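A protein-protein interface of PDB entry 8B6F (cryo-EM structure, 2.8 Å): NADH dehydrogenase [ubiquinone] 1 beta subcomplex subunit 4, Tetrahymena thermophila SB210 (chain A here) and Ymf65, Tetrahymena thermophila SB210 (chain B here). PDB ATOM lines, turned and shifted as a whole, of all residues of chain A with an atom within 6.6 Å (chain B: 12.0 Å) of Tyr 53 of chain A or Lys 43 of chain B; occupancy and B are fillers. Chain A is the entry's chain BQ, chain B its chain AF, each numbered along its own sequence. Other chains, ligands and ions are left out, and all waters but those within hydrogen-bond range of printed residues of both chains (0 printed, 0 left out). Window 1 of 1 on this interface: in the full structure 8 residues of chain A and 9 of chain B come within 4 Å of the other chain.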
ATOM      1  N   LEU A  49       7.296   7.411  14.893  1.00  0.00           N
ATOM      2  CA  LEU A  49       7.853   6.312  14.111  1.00  0.00           C
ATOM      3  C   LEU A  49       8.754   5.415  14.953  1.00  0.00           C
ATOM      4  O   LEU A  49       8.707   4.186  14.825  1.00  0.00           O
ATOM      5  CB  LEU A  49       8.624   6.860  12.910  1.00  0.00           C
ATOM      6  CG  LEU A  49       7.793   7.147  11.655  1.00  0.00           C
ATOM      7  CD1 LEU A  49       6.681   8.143  11.939  1.00  0.00           C
ATOM      8  CD2 LEU A  49       8.685   7.644  10.528  1.00  0.00           C
ATOM      9  N   ILE A  50       9.575   6.002  15.820  1.00  0.00           N
ATOM     10  CA  ILE A  50      10.564   5.233  16.567  1.00  0.00           C
ATOM     11  C   ILE A  50       9.985   4.771  17.896  1.00  0.00           C
ATOM     12  O   ILE A  50      10.713   4.256  18.751  1.00  0.00           O
ATOM     13  CB  ILE A  50      11.854   6.044  16.798  1.00  0.00           C
ATOM     14  CG1 ILE A  50      11.620   7.131  17.855  1.00  0.00           C
ATOM     15  CG2 ILE A  50      12.342   6.635  15.477  1.00  0.00           C
ATOM     16  CD1 ILE A  50      12.778   8.092  18.045  1.00  0.00           C
ATOM     17  N   TYR A  51       8.680   4.956  18.091  1.00  0.00           N
ATOM     18  CA  TYR A  51       8.046   4.499  19.320  1.00  0.00           C
ATOM     19  C   TYR A  51       8.350   3.026  19.556  1.00  0.00           C
ATOM     20  O   TYR A  51       8.232   2.200  18.649  1.00  0.00           O
ATOM     21  CB  TYR A  51       6.536   4.724  19.257  1.00  0.00           C
ATOM     22  CG  TYR A  51       5.816   4.229  20.489  1.00  0.00           C
ATOM     23  CD1 TYR A  51       5.895   4.925  21.687  1.00  0.00           C
ATOM     24  CD2 TYR A  51       5.063   3.065  20.456  1.00  0.00           C
ATOM     25  CE1 TYR A  51       5.243   4.476  22.816  1.00  0.00           C
ATOM     26  CE2 TYR A  51       4.406   2.607  21.582  1.00  0.00           C
ATOM     27  CZ  TYR A  51       4.502   3.319  22.758  1.00  0.00           C
ATOM     28  OH  TYR A  51       3.849   2.869  23.881  1.00  0.00           O
ATOM     29  N   GLY A  52       8.740   2.707  20.787  1.00  0.00           N
ATOM     30  CA  GLY A  52       9.181   1.373  21.125  1.00  0.00           C
ATOM     31  C   GLY A  52      10.653   1.123  20.893  1.00  0.00           C
ATOM     32  O   GLY A  52      11.134   0.029  21.215  1.00  0.00           O
ATOM     33  N   TYR A  53      11.383   2.097  20.352  1.00  0.00           N
ATOM     34  CA  TYR A  53      12.807   1.942  20.085  1.00  0.00           C
ATOM     35  C   TYR A  53      13.575   3.176  20.542  1.00  0.00           C
ATOM     36  O   TYR A  53      13.007   4.071  21.176  1.00  0.00           O
ATOM     37  CB  TYR A  53      13.043   1.689  18.593  1.00  0.00           C
ATOM     38  CG  TYR A  53      12.518   0.359  18.110  1.00  0.00           C
ATOM     39  CD1 TYR A  53      13.277  -0.797  18.236  1.00  0.00           C
ATOM     40  CD2 TYR A  53      11.266   0.261  17.519  1.00  0.00           C
ATOM     41  CE1 TYR A  53      12.801  -2.014  17.794  1.00  0.00           C
ATOM     42  CE2 TYR A  53      10.781  -0.951  17.073  1.00  0.00           C
ATOM     43  CZ  TYR A  53      11.554  -2.085  17.214  1.00  0.00           C
ATOM     44  OH  TYR A  53      11.074  -3.295  16.769  1.00  0.00           O
ATOM     45  N   THR A  54      14.863   3.229  20.224  1.00  0.00           N
ATOM     46  CA  THR A  54      15.725   4.344  20.578  1.00  0.00           C
ATOM     47  C   THR A  54      16.427   4.841  19.322  1.00  0.00           C
ATOM     48  O   THR A  54      16.602   4.100  18.352  1.00  0.00           O
ATOM     49  CB  THR A  54      16.752   3.931  21.649  1.00  0.00           C
ATOM     50  OG1 THR A  54      16.070   3.450  22.812  1.00  0.00           O
ATOM     51  CG2 THR A  54      17.641   5.089  22.043  1.00  0.00           C
ATOM     52  N   MET A  55      16.828   6.114  19.346  1.00  0.00           N
ATOM     53  CA  MET A  55      17.508   6.692  18.191  1.00  0.00           C
ATOM     54  C   MET A  55      18.803   5.950  17.890  1.00  0.00           C
ATOM     55  O   MET A  55      19.115   5.681  16.724  1.00  0.00           O
ATOM     56  CB  MET A  55      17.791   8.174  18.433  1.00  0.00           C
ATOM     57  CG  MET A  55      16.552   9.055  18.436  1.00  0.00           C
ATOM     58  SD  MET A  55      15.712   9.121  16.839  1.00  0.00           S
ATOM     59  CE  MET A  55      16.956   9.903  15.816  1.00  0.00           C
ATOM     60  N   GLU A  57      19.389   2.825  18.669  1.00  0.00           N
ATOM     61  CA  GLU A  57      19.034   1.487  18.209  1.00  0.00           C
ATOM     62  C   GLU A  57      18.668   1.485  16.730  1.00  0.00           C
ATOM     63  O   GLU A  57      19.058   0.575  15.990  1.00  0.00           O
ATOM     64  CB  GLU A  57      17.879   0.937  19.043  1.00  0.00           C
ATOM     65  CG  GLU A  57      18.261   0.598  20.472  1.00  0.00           C
ATOM     66  CD  GLU A  57      17.093   0.061  21.275  1.00  0.00           C
ATOM     67  OE1 GLU A  57      15.986  -0.053  20.711  1.00  0.00           O
ATOM     68  OE2 GLU A  57      17.283  -0.248  22.470  1.00  0.00           O
ATOM     69  N   LEU A  58      17.921   2.491  16.279  1.00  0.00           N
ATOM     70  CA  LEU A  58      17.427   2.510  14.905  1.00  0.00           C
ATOM     71  C   LEU A  58      18.439   3.128  13.944  1.00  0.00           C
ATOM     72  O   LEU A  58      18.881   2.475  12.994  1.00  0.00           O
ATOM     73  CB  LEU A  58      16.097   3.267  14.838  1.00  0.00           C
ATOM     74  CG  LEU A  58      14.922   2.646  15.594  1.00  0.00           C
ATOM     75  CD1 LEU A  58      13.687   3.495  15.399  1.00  0.00           C
ATOM     76  CD2 LEU A  58      14.656   1.217  15.150  1.00  0.00           C
ATOM     77  N   ASN B  36      12.398  19.993  27.347  1.00  0.00           N
ATOM     78  CA  ASN B  36      12.917  18.772  27.964  1.00  0.00           C
ATOM     79  C   ASN B  36      13.558  17.941  26.857  1.00  0.00           C
ATOM     80  O   ASN B  36      12.863  17.213  26.144  1.00  0.00           O
ATOM     81  CB  ASN B  36      11.810  18.008  28.676  1.00  0.00           C
ATOM     82  CG  ASN B  36      12.322  16.787  29.413  1.00  0.00           C
ATOM     83  OD1 ASN B  36      13.526  16.599  29.565  1.00  0.00           O
ATOM     84  ND2 ASN B  36      11.403  15.954  29.882  1.00  0.00           N
ATOM     85  N   LYS B  37      14.878  18.053  26.724  1.00  0.00           N
ATOM     86  CA  LYS B  37      15.586  17.370  25.651  1.00  0.00           C
ATOM     87  C   LYS B  37      15.537  15.858  25.835  1.00  0.00           C
ATOM     88  O   LYS B  37      15.596  15.348  26.958  1.00  0.00           O
ATOM     89  CB  LYS B  37      17.040  17.837  25.600  1.00  0.00           C
ATOM     90  CG  LYS B  37      17.867  17.165  24.516  1.00  0.00           C
ATOM     91  CD  LYS B  37      19.300  17.669  24.523  1.00  0.00           C
ATOM     92  CE  LYS B  37      20.133  16.958  23.469  1.00  0.00           C
ATOM     93  NZ  LYS B  37      21.553  17.407  23.482  1.00  0.00           N
ATOM     94  N   LYS B  38      15.427  15.143  24.718  1.00  0.00           N
ATOM     95  CA  LYS B  38      15.461  13.685  24.692  1.00  0.00           C
ATOM     96  C   LYS B  38      16.770  13.257  24.040  1.00  0.00           C
ATOM     97  O   LYS B  38      16.936  13.387  22.823  1.00  0.00           O
ATOM     98  CB  LYS B  38      14.259  13.124  23.933  1.00  0.00           C
ATOM     99  CG  LYS B  38      14.269  11.609  23.783  1.00  0.00           C
ATOM    100  CD  LYS B  38      13.057  11.124  23.005  1.00  0.00           C
ATOM    101  CE  LYS B  38      13.130   9.628  22.751  1.00  0.00           C
ATOM    102  NZ  LYS B  38      11.954   9.131  21.986  1.00  0.00           N
ATOM    103  N   ASN B  39      17.692  12.745  24.847  1.00  0.00           N
ATOM    104  CA  ASN B  39      18.972  12.290  24.328  1.00  0.00           C
ATOM    105  C   ASN B  39      18.778  11.091  23.409  1.00  0.00           C
ATOM    106  O   ASN B  39      17.811  10.333  23.533  1.00  0.00           O
ATOM    107  CB  ASN B  39      19.914  11.931  25.474  1.00  0.00           C
ATOM    108  CG  ASN B  39      20.153  13.096  26.409  1.00  0.00           C
ATOM    109  OD1 ASN B  39      19.845  13.028  27.597  1.00  0.00           O
ATOM    110  ND2 ASN B  39      20.704  14.179  25.873  1.00  0.00           N
ATOM    111  N   ASN B  40      19.712  10.922  22.470  1.00  0.00           N
ATOM    112  CA  ASN B  40      19.568   9.865  21.473  1.00  0.00           C
ATOM    113  C   ASN B  40      19.468   8.491  22.118  1.00  0.00           C
ATOM    114  O   ASN B  40      18.875   7.579  21.536  1.00  0.00           O
ATOM    115  CB  ASN B  40      20.736   9.904  20.489  1.00  0.00           C
ATOM    116  CG  ASN B  40      20.709  11.132  19.606  1.00  0.00           C
ATOM    117  OD1 ASN B  40      20.215  12.186  20.004  1.00  0.00           O
ATOM    118  ND2 ASN B  40      21.235  11.003  18.394  1.00  0.00           N
ATOM    119  N   TRP B  41      20.038   8.319  23.306  1.00  0.00           N
ATOM    120  CA  TRP B  41      19.938   7.058  24.024  1.00  0.00           C
ATOM    121  C   TRP B  41      18.692   6.961  24.897  1.00  0.00           C
ATOM    122  O   TRP B  41      18.422   5.885  25.440  1.00  0.00           O
ATOM    123  CB  TRP B  41      21.194   6.847  24.879  1.00  0.00           C
ATOM    124  CG  TRP B  41      21.437   7.936  25.875  1.00  0.00           C
ATOM    125  CD1 TRP B  41      20.937   8.020  27.139  1.00  0.00           C
ATOM    126  CD2 TRP B  41      22.249   9.103  25.685  1.00  0.00           C
ATOM    127  NE1 TRP B  41      21.389   9.166  27.746  1.00  0.00           N
ATOM    128  CE2 TRP B  41      22.194   9.846  26.876  1.00  0.00           C
ATOM    129  CE3 TRP B  41      23.016   9.589  24.623  1.00  0.00           C
ATOM    130  CZ2 TRP B  41      22.872  11.050  27.040  1.00  0.00           C
ATOM    131  CZ3 TRP B  41      23.692  10.786  24.786  1.00  0.00           C
ATOM    132  CH2 TRP B  41      23.615  11.503  25.987  1.00  0.00           C
ATOM    133  N   ASP B  42      17.937   8.045  25.052  1.00  0.00           N
ATOM    134  CA  ASP B  42      16.724   8.008  25.857  1.00  0.00           C
ATOM    135  C   ASP B  42      15.602   7.285  25.119  1.00  0.00           C
ATOM    136  O   ASP B  42      15.474   7.371  23.895  1.00  0.00           O
ATOM    137  CB  ASP B  42      16.271   9.422  26.217  1.00  0.00           C
ATOM    138  CG  ASP B  42      17.176  10.081  27.234  1.00  0.00           C
ATOM    139  OD1 ASP B  42      17.702   9.366  28.110  1.00  0.00           O
ATOM    140  OD2 ASP B  42      17.359  11.312  27.159  1.00  0.00           O
ATOM    141  N   LYS B  43      14.779   6.572  25.884  1.00  0.00           N
ATOM    142  CA  LYS B  43      13.645   5.826  25.356  1.00  0.00           C
ATOM    143  C   LYS B  43      12.363   6.386  25.955  1.00  0.00           C
ATOM    144  O   LYS B  43      12.283   6.590  27.171  1.00  0.00           O
ATOM    145  CB  LYS B  43      13.777   4.334  25.670  1.00  0.00           C
ATOM    146  CG  LYS B  43      12.664   3.470  25.101  1.00  0.00           C
ATOM    147  CD  LYS B  43      12.895   1.999  25.421  1.00  0.00           C
ATOM    148  CE  LYS B  43      11.773   1.133  24.876  1.00  0.00           C
ATOM    149  NZ  LYS B  43      11.996  -0.312  25.158  1.00  0.00           N
ATOM    150  N   SER B  44      11.369   6.634  25.107  1.00  0.00           N
ATOM    151  CA  SER B  44      10.102   7.224  25.526  1.00  0.00           C
ATOM    152  C   SER B  44       9.065   6.124  25.699  1.00  0.00           C
ATOM    153  O   SER B  44       8.787   5.374  24.757  1.00  0.00           O
ATOM    154  CB  SER B  44       9.614   8.259  24.513  1.00  0.00           C
ATOM    155  OG  SER B  44      10.500   9.361  24.441  1.00  0.00           O
ATOM    156  N   ILE B  45       8.493   6.032  26.900  1.00  0.00           N
ATOM    157  CA  ILE B  45       7.447   5.047  27.149  1.00  0.00           C
ATOM    158  C   ILE B  45       6.200   5.379  26.339  1.00  0.00           C
ATOM    159  O   ILE B  45       5.490   4.482  25.871  1.00  0.00           O
ATOM    160  CB  ILE B  45       7.147   4.961  28.657  1.00  0.00           C
ATOM    161  CG1 ILE B  45       6.197   3.795  28.939  1.00  0.00           C
ATOM    162  CG2 ILE B  45       6.566   6.277  29.167  1.00  0.00           C
ATOM    163  CD1 ILE B  45       5.964   3.529  30.413  1.00  0.00           C
ATOM    164  N   SER B  46       5.912   6.666  26.167  1.00  0.00           N
ATOM    165  CA  SER B  46       4.762   7.118  25.400  1.00  0.00           C
ATOM    166  C   SER B  46       5.186   8.285  24.520  1.00  0.00           C
ATOM    167  O   SER B  46       6.212   8.927  24.756  1.00  0.00           O
ATOM    168  CB  SER B  46       3.599   7.525  26.314  1.00  0.00           C
ATOM    169  OG  SER B  46       4.006   8.496  27.261  1.00  0.00           O
ATOM    170  N   VAL B  47       4.388   8.547  23.488  1.00  0.00           N
ATOM    171  CA  VAL B  47       4.670   9.657  22.585  1.00  0.00           C
ATOM    172  C   VAL B  47       4.369  10.970  23.296  1.00  0.00           C
ATOM    173  O   VAL B  47       3.294  11.146  23.882  1.00  0.00           O
ATOM    174  CB  VAL B  47       3.853   9.521  21.291  1.00  0.00           C
ATOM    175  CG1 VAL B  47       4.060  10.729  20.390  1.00  0.00           C
ATOM    176  CG2 VAL B  47       4.229   8.243  20.560  1.00  0.00           C
ATOM    177  N   LYS B  48       5.319  11.900  23.242  1.00  0.00           N
ATOM    178  CA  LYS B  48       5.159  13.173  23.930  1.00  0.00           C
ATOM    179  C   LYS B  48       3.979  13.950  23.363  1.00  0.00           C
ATOM    180  O   LYS B  48       3.762  13.991  22.149  1.00  0.00           O
ATOM    181  CB  LYS B  48       6.437  14.004  23.807  1.00  0.00           C
ATOM    182  CG  LYS B  48       6.333  15.396  24.412  1.00  0.00           C
ATOM    183  CD  LYS B  48       7.650  16.144  24.315  1.00  0.00           C
ATOM    184  CE  LYS B  48       7.539  17.534  24.917  1.00  0.00           C
ATOM    185  NZ  LYS B  48       8.822  18.282  24.817  1.00  0.00           N
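N of Met 55 of chain A lies within hydrogen-bond range of O of Asn 40 of chain B, 3.3 Å away. The backbone carbonyl oxygen of Ile 45 of chain B sits at hydrogen-bond distance from the side-chain hydroxyl of Tyr 51 of chain A (3.0 Å).
Of the 9 printed residues of chain A, 5 touch a printed residue of chain B. Hydrophobic or aromatic side chains of chain A that line the printed part of chain B: Tyr 51 and Met 55. Among the printed residues, no Asp or Glu carboxylate lies within 4 Å of a Lys or Arg side-chain nitrogen of the other chain.
N of Asn 39 of chain B lies within hydrogen-bond range of OD2 of Asp 42 of chain B.
Among the printed residues, merely in contact across the chains: Thr 54 of chain A with Asn 40 of chain B (2.8 Å), Thr 54 of chain A with Trp 41 of chain B (3.6 Å), Thr 54 of chain A with Asp 42 of chain B (3.7 Å), Tyr 51 of chain A with Ser 46 of chain B (3.7 Å), Thr 54 of chain A with Lys 43 of chain B (3.8 Å), Gly 52 of chain A with Lys 43 of chain B (3.9 Å), Tyr 51 of chain A with Val 47 of chain B (3.9 Å) and Tyr 53 of chain A with Lys 43 of chain B (3.99 Å).
Leu 49 of chain A touches none of the printed residues of chain B. No residue of chain B comes within 4 Å of Ile 50 of chain A. Gly 52 of chain A touches just one residue of chain B: Lys 43 (3.9 Å). Of the printed residues of chain B, Tyr 53 of chain A touches Lys 43 (3.99 Å). Printed residues of chain B within 4 Å of Thr 54 of chain A: Asn 40, Trp 41, Asp 42 and Lys 43. No residue of chain B comes within 4 Å of Glu 57 of chain A. Of the printed residues of chain A, Trp 41 of chain B touches Thr 54. Printed residues of chain A within 4 Å of Asp 42 of chain B: Thr 54 (3.7 Å). Printed residues of chain A within 4 Å of Lys 43 of chain B: Gly 52, Tyr 53 and Thr 54. The nearest printed residue of chain A that does not touch Asn 40 of chain B is Glu 57 of chain A (5.6 Å).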
